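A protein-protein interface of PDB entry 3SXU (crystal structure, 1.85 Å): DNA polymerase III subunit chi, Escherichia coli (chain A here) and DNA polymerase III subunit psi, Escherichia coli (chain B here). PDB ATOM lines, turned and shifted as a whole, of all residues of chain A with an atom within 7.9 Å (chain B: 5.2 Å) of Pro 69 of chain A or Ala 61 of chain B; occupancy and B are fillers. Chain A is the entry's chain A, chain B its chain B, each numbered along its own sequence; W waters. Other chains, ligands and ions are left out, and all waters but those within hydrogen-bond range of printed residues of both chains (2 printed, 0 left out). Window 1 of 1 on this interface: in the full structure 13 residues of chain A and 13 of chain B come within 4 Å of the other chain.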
ATOM      1  N   ALA A  32      23.826 -17.212  10.076  1.00  0.00           N
ATOM      2  CA  ALA A  32      22.710 -18.178  10.153  1.00  0.00           C
ATOM      3  C   ALA A  32      22.933 -19.224  11.252  1.00  0.00           C
ATOM      4  O   ALA A  32      22.021 -19.521  12.043  1.00  0.00           O
ATOM      5  CB  ALA A  32      22.474 -18.850   8.795  1.00  0.00           C
ATOM      6  N   ALA A  33      24.151 -19.763  11.321  1.00  0.00           N
ATOM      7  CA  ALA A  33      24.476 -20.771  12.334  1.00  0.00           C
ATOM      8  C   ALA A  33      24.354 -20.186  13.743  1.00  0.00           C
ATOM      9  O   ALA A  33      23.744 -20.796  14.624  1.00  0.00           O
ATOM     10  CB  ALA A  33      25.869 -21.327  12.110  1.00  0.00           C
ATOM     11  N   TRP A  36      20.572 -19.538  14.609  1.00  0.00           N
ATOM     12  CA  TRP A  36      19.891 -20.810  14.894  1.00  0.00           C
ATOM     13  C   TRP A  36      20.310 -21.379  16.267  1.00  0.00           C
ATOM     14  O   TRP A  36      19.468 -21.876  17.033  1.00  0.00           O
ATOM     15  CB  TRP A  36      20.123 -21.839  13.773  1.00  0.00           C
ATOM     16  CG  TRP A  36      19.644 -23.189  14.192  1.00  0.00           C
ATOM     17  CD1 TRP A  36      18.346 -23.562  14.416  1.00  0.00           C
ATOM     18  CD2 TRP A  36      20.453 -24.328  14.506  1.00  0.00           C
ATOM     19  NE1 TRP A  36      18.297 -24.875  14.825  1.00  0.00           N
ATOM     20  CE2 TRP A  36      19.573 -25.371  14.886  1.00  0.00           C
ATOM     21  CE3 TRP A  36      21.835 -24.578  14.482  1.00  0.00           C
ATOM     22  CZ2 TRP A  36      20.029 -26.647  15.255  1.00  0.00           C
ATOM     23  CZ3 TRP A  36      22.291 -25.849  14.837  1.00  0.00           C
ATOM     24  CH2 TRP A  36      21.388 -26.864  15.227  1.00  0.00           C
ATOM     25  N   ARG A  37      21.604 -21.288  16.583  1.00  0.00           N
ATOM     26  CA  ARG A  37      22.098 -21.766  17.873  1.00  0.00           C
ATOM     27  C   ARG A  37      21.559 -20.964  19.061  1.00  0.00           C
ATOM     28  O   ARG A  37      21.516 -21.476  20.183  1.00  0.00           O
ATOM     29  CB  ARG A  37      23.625 -21.795  17.893  1.00  0.00           C
ATOM     30  CG  ARG A  37      24.203 -22.964  17.096  1.00  0.00           C
ATOM     31  CD  ARG A  37      25.698 -22.861  17.008  1.00  0.00           C
ATOM     32  NE  ARG A  37      26.297 -24.079  16.455  1.00  0.00           N
ATOM     33  CZ  ARG A  37      27.448 -24.106  15.791  1.00  0.00           C
ATOM     34  NH1 ARG A  37      28.121 -22.977  15.563  1.00  0.00           N
ATOM     35  NH2 ARG A  37      27.931 -25.261  15.359  1.00  0.00           N
ATOM     36  N   VAL A  42      15.324 -19.147  11.101  1.00  0.00           N
ATOM     37  CA  VAL A  42      15.998 -18.189  10.233  1.00  0.00           C
ATOM     38  C   VAL A  42      15.484 -18.321   8.811  1.00  0.00           C
ATOM     39  O   VAL A  42      15.306 -19.440   8.315  1.00  0.00           O
ATOM     40  CB  VAL A  42      17.523 -18.449  10.225  1.00  0.00           C
ATOM     41  CG1 VAL A  42      18.251 -17.454   9.317  1.00  0.00           C
ATOM     42  CG2 VAL A  42      18.088 -18.403  11.645  1.00  0.00           C
ATOM     43  N   ASP A  56      22.757 -23.587   0.133  1.00  0.00           N
ATOM     44  CA  ASP A  56      22.251 -24.875   0.609  1.00  0.00           C
ATOM     45  C   ASP A  56      23.405 -25.883   0.752  1.00  0.00           C
ATOM     46  O   ASP A  56      23.450 -26.653   1.722  1.00  0.00           O
ATOM     47  CB  ASP A  56      21.138 -25.413  -0.303  1.00  0.00           C
ATOM     48  CG  ASP A  56      20.374 -26.574   0.321  1.00  0.00           C
ATOM     49  OD1 ASP A  56      20.095 -26.553   1.526  1.00  0.00           O
ATOM     50  OD2 ASP A  56      20.037 -27.529  -0.399  1.00  0.00           O
ATOM     51  N   LEU A  59      26.092 -24.337   3.754  1.00  0.00           N
ATOM     52  CA  LEU A  59      25.692 -24.427   5.172  1.00  0.00           C
ATOM     53  C   LEU A  59      25.864 -25.804   5.797  1.00  0.00           C
ATOM     54  O   LEU A  59      25.744 -25.945   7.012  1.00  0.00           O
ATOM     55  CB  LEU A  59      24.258 -23.924   5.390  1.00  0.00           C
ATOM     56  CG  LEU A  59      24.010 -22.584   6.073  1.00  0.00           C
ATOM     57  CD1 LEU A  59      22.508 -22.466   6.344  1.00  0.00           C
ATOM     58  CD2 LEU A  59      24.799 -22.434   7.380  1.00  0.00           C
ATOM     59  N   TRP A  60      26.141 -26.827   4.983  1.00  0.00           N
ATOM     60  CA  TRP A  60      26.547 -28.123   5.524  1.00  0.00           C
ATOM     61  C   TRP A  60      28.027 -28.175   5.893  1.00  0.00           C
ATOM     62  O   TRP A  60      28.459 -29.098   6.605  1.00  0.00           O
ATOM     63  CB  TRP A  60      26.204 -29.281   4.566  1.00  0.00           C
ATOM     64  CG  TRP A  60      24.726 -29.521   4.472  1.00  0.00           C
ATOM     65  CD1 TRP A  60      23.944 -29.398   3.357  1.00  0.00           C
ATOM     66  CD2 TRP A  60      23.847 -29.890   5.541  1.00  0.00           C
ATOM     67  NE1 TRP A  60      22.632 -29.676   3.666  1.00  0.00           N
ATOM     68  CE2 TRP A  60      22.545 -29.982   5.000  1.00  0.00           C
ATOM     69  CE3 TRP A  60      24.031 -30.137   6.916  1.00  0.00           C
ATOM     70  CZ2 TRP A  60      21.429 -30.308   5.778  1.00  0.00           C
ATOM     71  CZ3 TRP A  60      22.927 -30.468   7.687  1.00  0.00           C
ATOM     72  CH2 TRP A  60      21.639 -30.545   7.117  1.00  0.00           C
ATOM     73  N   SER A  66      30.059 -28.513  12.351  1.00  0.00           N
ATOM     74  CA  SER A  66      28.768 -28.045  12.844  1.00  0.00           C
ATOM     75  C   SER A  66      27.652 -28.703  12.060  1.00  0.00           C
ATOM     76  O   SER A  66      27.801 -28.958  10.866  1.00  0.00           O
ATOM     77  CB  SER A  66      28.662 -26.528  12.654  1.00  0.00           C
ATOM     78  OG  SER A  66      29.692 -25.857  13.364  1.00  0.00           O
ATOM     79  N   PHE A  67      26.530 -28.937  12.729  1.00  0.00           N
ATOM     80  CA  PHE A  67      25.344 -29.511  12.092  1.00  0.00           C
ATOM     81  C   PHE A  67      24.261 -28.454  12.156  1.00  0.00           C
ATOM     82  O   PHE A  67      23.641 -28.256  13.207  1.00  0.00           O
ATOM     83  CB  PHE A  67      24.921 -30.772  12.846  1.00  0.00           C
ATOM     84  CG  PHE A  67      23.712 -31.462  12.272  1.00  0.00           C
ATOM     85  CD1 PHE A  67      23.849 -32.374  11.229  1.00  0.00           C
ATOM     86  CD2 PHE A  67      22.445 -31.229  12.802  1.00  0.00           C
ATOM     87  CE1 PHE A  67      22.724 -33.044  10.702  1.00  0.00           C
ATOM     88  CE2 PHE A  67      21.309 -31.887  12.277  1.00  0.00           C
ATOM     89  CZ  PHE A  67      21.458 -32.798  11.232  1.00  0.00           C
ATOM     90  N   VAL A  68      24.056 -27.756  11.044  1.00  0.00           N
ATOM     91  CA  VAL A  68      23.073 -26.672  10.989  1.00  0.00           C
ATOM     92  C   VAL A  68      21.942 -27.099  10.063  1.00  0.00           C
ATOM     93  O   VAL A  68      22.092 -27.063   8.846  1.00  0.00           O
ATOM     94  CB  VAL A  68      23.702 -25.353  10.497  1.00  0.00           C
ATOM     95  CG1 VAL A  68      22.672 -24.213  10.526  1.00  0.00           C
ATOM     96  CG2 VAL A  68      24.933 -25.004  11.345  1.00  0.00           C
ATOM     97  N   PRO A  69      20.810 -27.518  10.643  1.00  0.00           N
ATOM     98  CA  PRO A  69      19.737 -28.102   9.832  1.00  0.00           C
ATOM     99  C   PRO A  69      19.077 -27.044   8.970  1.00  0.00           C
ATOM    100  O   PRO A  69      18.652 -26.000   9.473  1.00  0.00           O
ATOM    101  CB  PRO A  69      18.767 -28.646  10.881  1.00  0.00           C
ATOM    102  CG  PRO A  69      18.972 -27.746  12.071  1.00  0.00           C
ATOM    103  CD  PRO A  69      20.459 -27.476  12.073  1.00  0.00           C
ATOM    104  N   HIS A  70      19.008 -27.303   7.672  1.00  0.00           N
ATOM    105  CA  HIS A  70      18.535 -26.289   6.739  1.00  0.00           C
ATOM    106  C   HIS A  70      18.079 -26.939   5.454  1.00  0.00           C
ATOM    107  O   HIS A  70      18.498 -28.060   5.126  1.00  0.00           O
ATOM    108  CB  HIS A  70      19.638 -25.263   6.442  1.00  0.00           C
ATOM    109  CG  HIS A  70      20.776 -25.819   5.652  1.00  0.00           C
ATOM    110  ND1 HIS A  70      21.801 -26.533   6.231  1.00  0.00           N
ATOM    111  CD2 HIS A  70      21.036 -25.792   4.323  1.00  0.00           C
ATOM    112  CE1 HIS A  70      22.646 -26.920   5.293  1.00  0.00           C
ATOM    113  NE2 HIS A  70      22.209 -26.479   4.127  1.00  0.00           N
ATOM    114  N   ASN A  71      17.226 -26.223   4.729  1.00  0.00           N
ATOM    115  CA  ASN A  71      16.746 -26.664   3.421  1.00  0.00           C
ATOM    116  C   ASN A  71      16.380 -25.480   2.566  1.00  0.00           C
ATOM    117  O   ASN A  71      16.131 -24.389   3.079  1.00  0.00           O
ATOM    118  CB  ASN A  71      15.488 -27.523   3.555  1.00  0.00           C
ATOM    119  CG  ASN A  71      15.786 -28.932   4.010  1.00  0.00           C
ATOM    120  OD1 ASN A  71      16.314 -29.758   3.250  1.00  0.00           O
ATOM    121  ND2 ASN A  71      15.429 -29.226   5.241  1.00  0.00           N
ATOM    122  N   PRO A  77      11.166 -30.556   6.509  1.00  0.00           N
ATOM    123  CA  PRO A  77       9.965 -31.003   7.220  1.00  0.00           C
ATOM    124  C   PRO A  77       8.818 -29.992   7.135  1.00  0.00           C
ATOM    125  O   PRO A  77       9.018 -28.871   6.655  1.00  0.00           O
ATOM    126  CB  PRO A  77      10.450 -31.156   8.667  1.00  0.00           C
ATOM    127  CG  PRO A  77      11.589 -30.191   8.802  1.00  0.00           C
ATOM    128  CD  PRO A  77      12.165 -29.959   7.422  1.00  0.00           C
ATOM    129  N   GLY A  80       8.923 -26.173   7.333  1.00  0.00           N
ATOM    130  CA  GLY A  80      10.274 -25.837   6.893  1.00  0.00           C
ATOM    131  C   GLY A  80      11.341 -26.158   7.922  1.00  0.00           C
ATOM    132  O   GLY A  80      11.050 -26.358   9.114  1.00  0.00           O
ATOM    133  N   ALA A  81      12.583 -26.199   7.451  1.00  0.00           N
ATOM    134  CA  ALA A  81      13.755 -26.435   8.301  1.00  0.00           C
ATOM    135  C   ALA A  81      14.023 -25.248   9.230  1.00  0.00           C
ATOM    136  O   ALA A  81      13.532 -24.149   8.977  1.00  0.00           O
ATOM    137  CB  ALA A  81      14.969 -26.708   7.429  1.00  0.00           C
ATOM    138  N   PRO A  82      14.806 -25.459  10.312  1.00  0.00           N
ATOM    139  CA  PRO A  82      15.094 -24.334  11.205  1.00  0.00           C
ATOM    140  C   PRO A  82      15.730 -23.140  10.482  1.00  0.00           C
ATOM    141  O   PRO A  82      15.423 -21.987  10.797  1.00  0.00           O
ATOM    142  CB  PRO A  82      16.058 -24.944  12.225  1.00  0.00           C
ATOM    143  CG  PRO A  82      15.608 -26.386  12.316  1.00  0.00           C
ATOM    144  CD  PRO A  82      15.306 -26.733  10.864  1.00  0.00           C
ATOM    145  N   VAL A  83      16.610 -23.421   9.526  1.00  0.00           N
ATOM    146  CA  VAL A  83      17.107 -22.395   8.611  1.00  0.00           C
ATOM    147  C   VAL A  83      16.573 -22.711   7.218  1.00  0.00           C
ATOM    148  O   VAL A  83      16.782 -23.813   6.704  1.00  0.00           O
ATOM    149  CB  VAL A  83      18.647 -22.342   8.609  1.00  0.00           C
ATOM    150  CG1 VAL A  83      19.156 -21.268   7.648  1.00  0.00           C
ATOM    151  CG2 VAL A  83      19.164 -22.079  10.033  1.00  0.00           C
ATOM    152  N   GLU A  84      15.871 -21.752   6.620  1.00  0.00           N
ATOM    153  CA  GLU A  84      15.300 -21.952   5.291  1.00  0.00           C
ATOM    154  C   GLU A  84      15.909 -20.962   4.320  1.00  0.00           C
ATOM    155  O   GLU A  84      16.113 -19.790   4.661  1.00  0.00           O
ATOM    156  CB  GLU A  84      13.783 -21.788   5.321  1.00  0.00           C
ATOM    157  CG  GLU A  84      13.126 -21.992   3.957  1.00  0.00           C
ATOM    158  CD  GLU A  84      11.625 -22.075   4.040  1.00  0.00           C
ATOM    159  OE1 GLU A  84      11.098 -23.141   4.433  1.00  0.00           O
ATOM    160  OE2 GLU A  84      10.968 -21.069   3.703  1.00  0.00           O
ATOM    161  N   ARG A  96       9.024 -17.312  11.262  1.00  0.00           N
ATOM    162  CA  ARG A  96      10.471 -17.154  11.346  1.00  0.00           C
ATOM    163  C   ARG A  96      10.826 -15.885  12.096  1.00  0.00           C
ATOM    164  O   ARG A  96      10.088 -14.898  12.048  1.00  0.00           O
ATOM    165  CB  ARG A  96      11.115 -17.240   9.955  1.00  0.00           C
ATOM    166  CG  ARG A  96      10.968 -18.653   9.412  1.00  0.00           C
ATOM    167  CD  ARG A  96      11.642 -18.966   8.090  1.00  0.00           C
ATOM    168  NE  ARG A  96      11.295 -20.351   7.772  1.00  0.00           N
ATOM    169  CZ  ARG A  96      11.941 -21.418   8.239  1.00  0.00           C
ATOM    170  NH1 ARG A  96      13.035 -21.276   8.994  1.00  0.00           N
ATOM    171  NH2 ARG A  96      11.507 -22.634   7.926  1.00  0.00           N
ATOM    172  N   SER B  56      25.478 -31.439  20.594  1.00  0.00           N
ATOM    173  CA  SER B  56      24.568 -30.342  20.929  1.00  0.00           C
ATOM    174  C   SER B  56      23.746 -29.886  19.722  1.00  0.00           C
ATOM    175  O   SER B  56      22.531 -29.696  19.829  1.00  0.00           O
ATOM    176  CB  SER B  56      25.341 -29.154  21.512  1.00  0.00           C
ATOM    177  OG  SER B  56      25.802 -29.438  22.819  1.00  0.00           O
ATOM    178  N   ASP B  57      24.414 -29.718  18.581  1.00  0.00           N
ATOM    179  CA  ASP B  57      23.759 -29.286  17.342  1.00  0.00           C
ATOM    180  C   ASP B  57      22.675 -30.285  16.912  1.00  0.00           C
ATOM    181  O   ASP B  57      21.571 -29.893  16.544  1.00  0.00           O
ATOM    182  CB  ASP B  57      24.765 -29.156  16.188  1.00  0.00           C
ATOM    183  CG  ASP B  57      25.628 -27.908  16.256  1.00  0.00           C
ATOM    184  OD1 ASP B  57      25.334 -26.948  17.008  1.00  0.00           O
ATOM    185  OD2 ASP B  57      26.637 -27.884  15.506  1.00  0.00           O
ATOM    186  N   VAL B  58      23.002 -31.576  16.937  1.00  0.00           N
ATOM    187  CA  VAL B  58      22.030 -32.599  16.543  1.00  0.00           C
ATOM    188  C   VAL B  58      20.843 -32.611  17.518  1.00  0.00           C
ATOM    189  O   VAL B  58      19.680 -32.664  17.094  1.00  0.00           O
ATOM    190  CB  VAL B  58      22.693 -33.997  16.384  1.00  0.00           C
ATOM    191  CG1 VAL B  58      21.645 -35.082  16.088  1.00  0.00           C
ATOM    192  CG2 VAL B  58      23.702 -33.975  15.230  1.00  0.00           C
ATOM    193  N   LEU B  59      21.125 -32.542  18.817  1.00  0.00           N
ATOM    194  CA  LEU B  59      20.043 -32.490  19.803  1.00  0.00           C
ATOM    195  C   LEU B  59      19.160 -31.264  19.570  1.00  0.00           C
ATOM    196  O   LEU B  59      17.933 -31.364  19.619  1.00  0.00           O
ATOM    197  CB  LEU B  59      20.592 -32.506  21.242  1.00  0.00           C
ATOM    198  CG  LEU B  59      21.323 -33.788  21.663  1.00  0.00           C
ATOM    199  CD1 LEU B  59      21.757 -33.680  23.131  1.00  0.00           C
ATOM    200  CD2 LEU B  59      20.457 -35.026  21.440  1.00  0.00           C
ATOM    201  N   ARG B  60      19.784 -30.115  19.302  1.00  0.00           N
ATOM    202  CA  ARG B  60      19.034 -28.884  19.016  1.00  0.00           C
ATOM    203  C   ARG B  60      18.126 -29.070  17.787  1.00  0.00           C
ATOM    204  O   ARG B  60      16.962 -28.656  17.807  1.00  0.00           O
ATOM    205  CB  ARG B  60      19.985 -27.696  18.806  1.00  0.00           C
ATOM    206  CG  ARG B  60      19.309 -26.313  18.897  1.00  0.00           C
ATOM    207  CD  ARG B  60      20.290 -25.165  18.617  1.00  0.00           C
ATOM    208  NE  ARG B  60      21.414 -25.155  19.560  1.00  0.00           N
ATOM    209  CZ  ARG B  60      22.651 -25.562  19.264  1.00  0.00           C
ATOM    210  NH1 ARG B  60      22.951 -25.998  18.046  1.00  0.00           N
ATOM    211  NH2 ARG B  60      23.601 -25.524  20.188  1.00  0.00           N
ATOM    212  N   ALA B  61      18.663 -29.697  16.738  1.00  0.00           N
ATOM    213  CA  ALA B  61      17.904 -29.983  15.513  1.00  0.00           C
ATOM    214  C   ALA B  61      16.708 -30.900  15.776  1.00  0.00           C
ATOM    215  O   ALA B  61      15.656 -30.755  15.140  1.00  0.00           O
ATOM    216  CB  ALA B  61      18.810 -30.607  14.466  1.00  0.00           C
ATOM    217  N   LEU B  62      16.887 -31.863  16.681  1.00  0.00           N
ATOM    218  CA  LEU B  62      15.807 -32.786  17.072  1.00  0.00           C
ATOM    219  C   LEU B  62      14.824 -32.169  18.064  1.00  0.00           C
ATOM    220  O   LEU B  62      13.762 -32.751  18.352  1.00  0.00           O
ATOM    221  CB  LEU B  62      16.393 -34.075  17.661  1.00  0.00           C
ATOM    222  CG  LEU B  62      17.282 -34.945  16.768  1.00  0.00           C
ATOM    223  CD1 LEU B  62      17.934 -36.055  17.584  1.00  0.00           C
ATOM    224  CD2 LEU B  62      16.487 -35.523  15.593  1.00  0.00           C
ATOM    225  N   THR B  63      15.171 -30.985  18.567  1.00  0.00           N
ATOM    226  CA  THR B  63      14.427 -30.277  19.629  1.00  0.00           C
ATOM    227  C   THR B  63      14.364 -31.114  20.910  1.00  0.00           C
ATOM    228  O   THR B  63      13.346 -31.144  21.608  1.00  0.00           O
ATOM    229  CB  THR B  63      12.995 -29.774  19.195  1.00  0.00           C
ATOM    230  OG1 THR B  63      12.084 -30.878  19.097  1.00  0.00           O
ATOM    231  CG2 THR B  63      13.053 -29.037  17.857  1.00  0.00           C
ATOM    232  N   TRP B 123      20.409 -35.327   8.323  1.00  0.00           N
ATOM    233  CA  TRP B 123      19.251 -34.436   8.337  1.00  0.00           C
ATOM    234  C   TRP B 123      18.130 -34.996   7.457  1.00  0.00           C
ATOM    235  O   TRP B 123      16.954 -34.934   7.820  1.00  0.00           O
ATOM    236  CB  TRP B 123      19.629 -33.010   7.903  1.00  0.00           C
ATOM    237  CG  TRP B 123      18.454 -32.042   7.886  1.00  0.00           C
ATOM    238  CD1 TRP B 123      17.992 -31.337   6.804  1.00  0.00           C
ATOM    239  CD2 TRP B 123      17.596 -31.687   8.988  1.00  0.00           C
ATOM    240  NE1 TRP B 123      16.909 -30.571   7.167  1.00  0.00           N
ATOM    241  CE2 TRP B 123      16.644 -30.764   8.495  1.00  0.00           C
ATOM    242  CE3 TRP B 123      17.536 -32.065  10.339  1.00  0.00           C
ATOM    243  CZ2 TRP B 123      15.631 -30.214   9.305  1.00  0.00           C
ATOM    244  CZ3 TRP B 123      16.535 -31.506  11.151  1.00  0.00           C
ATOM    245  CH2 TRP B 123      15.597 -30.592  10.624  1.00  0.00           C
ATOM    246  N   PHE B 134       9.054 -34.534  15.339  1.00  0.00           N
ATOM    247  CA  PHE B 134       8.386 -33.240  15.444  1.00  0.00           C
ATOM    248  C   PHE B 134       6.865 -33.426  15.465  1.00  0.00           C
ATOM    249  O   PHE B 134       6.177 -32.972  14.550  1.00  0.00           O
ATOM    250  CB  PHE B 134       8.794 -32.328  14.276  1.00  0.00           C
ATOM    251  CG  PHE B 134      10.287 -32.289  14.016  1.00  0.00           C
ATOM    252  CD1 PHE B 134      10.798 -32.646  12.770  1.00  0.00           C
ATOM    253  CD2 PHE B 134      11.173 -31.896  15.015  1.00  0.00           C
ATOM    254  CE1 PHE B 134      12.178 -32.604  12.520  1.00  0.00           C
ATOM    255  CE2 PHE B 134      12.551 -31.864  14.778  1.00  0.00           C
ATOM    256  CZ  PHE B 134      13.049 -32.215  13.530  1.00  0.00           C
HETATM  257  O   HOH W   1      29.403 -27.916  16.471  1.00  0.00           O
HETATM  258  O   HOH W   2      16.066 -26.747  15.660  1.00  0.00           O
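Hydrophobic or aromatic side chains of chain B within 4 Å of the printed part of chain A: Val 58, Ala 61 and Trp 123.
Of the 21 printed residues of chain A, 10 touch a printed residue of chain B.
Printed residues of chain A that touch a printed residue of chain B: Trp 36, Arg 37, Trp 60, Ser 66, Phe 67, Pro 69, His 70, Asn 71, Pro 77 and Pro 82.
Among the printed residues, Asp or Glu carboxylates within 4 Å of a Lys or Arg side-chain nitrogen of the other chain: Arg 37 of chain A with Asp 57 of chain B.
The backbone NH (N) of Phe 67 of chain A is in hydrogen-bond range of the side-chain carboxylate (OD2) of Asp 57 of chain B (3.0 Å).
NH2 of Arg 37 of chain A is in salt-bridge range of OD2 of Asp 57 of chain B, at 2.9 Å.
The side-chain amide nitrogen (ND2) of Asn 71 of chain A lies close to the indole nitrogen (NE1) of Trp 123 of chain B, at 2.8 Å.
Among the printed residues, merely in contact across the chains: Trp 36 of chain A with Asp 57 of chain B, Trp 36 of chain A with Arg 60 of chain B, Trp 36 of chain A with Ala 61 of chain B, Arg 37 of chain A with Arg 60 of chain B, Trp 60 of chain A with Trp 123 of chain B, Ser 66 of chain A with Asp 57 of chain B, Phe 67 of chain A with Val 58 of chain B, Phe 67 of chain A with Ala 61 of chain B, Phe 67 of chain A with Trp 123 of chain B, Pro 69 of chain A with Ala 61 of chain B, Pro 69 of chain A with Trp 123 of chain B, His 70 of chain A with Trp 123 of chain B, Pro 77 of chain A with Trp 123 of chain B and Pro 82 of chain A with Trp 123 of chain B.
NE1 of Trp 60 of chain A lies close to NE2 of His 70 of chain A (3.3 Å).
OD1 of Asp 57 of chain B lies within salt-bridge range of NH1 of Arg 60 of chain B (2.8 Å).
The guanidinium group (NH1) of Arg 96 of chain A is in hydrogen-bond range of the backbone carbonyl oxygen (O) of Pro 82 of chain A, 3.1 Å away.
The backbone carbonyl oxygen of Val 68 of chain A sits at hydrogen-bond distance from a ring nitrogen (ND1) of His 70 of chain A (2.7 Å).
N of Asn 71 of chain A sits at hydrogen-bond distance from O of Val 83 of chain A, 3.1 Å away.
O of Pro 82 of chain A lies within hydrogen-bond range of N of Val 42 of chain A, at 2.9 Å.
Water W1 bridges OD2 of Asp 57 of chain B (2.9 Å) and NH2 of Arg 37 of chain A (3.2 Å).
Water W2 lies within hydrogen-bond range of the backbone carbonyl oxygen of Arg 60 of chain B and the indole nitrogen of Trp 36 of chain A.
Of the printed residues of chain B, Ser 66 of chain A touches Asp 57.
Of the printed residues of chain B, Phe 67 of chain A touches Asp 57, Val 58, Ala 61 and Trp 123.
Pro 69 of chain A touches two residues of chain B.
Printed residues of chain B within 4 Å of His 70 of chain A: Trp 123 (3.6 Å).
Of the printed residues of chain B, Asn 71 of chain A touches Trp 123.
Ala 61 of chain B touches just these residues of chain A: Trp 36, Phe 67 and Pro 69.
The nearest printed residue of chain B that does not touch Pro 69 of chain A is Asp 57 of chain B (5.2 Å).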
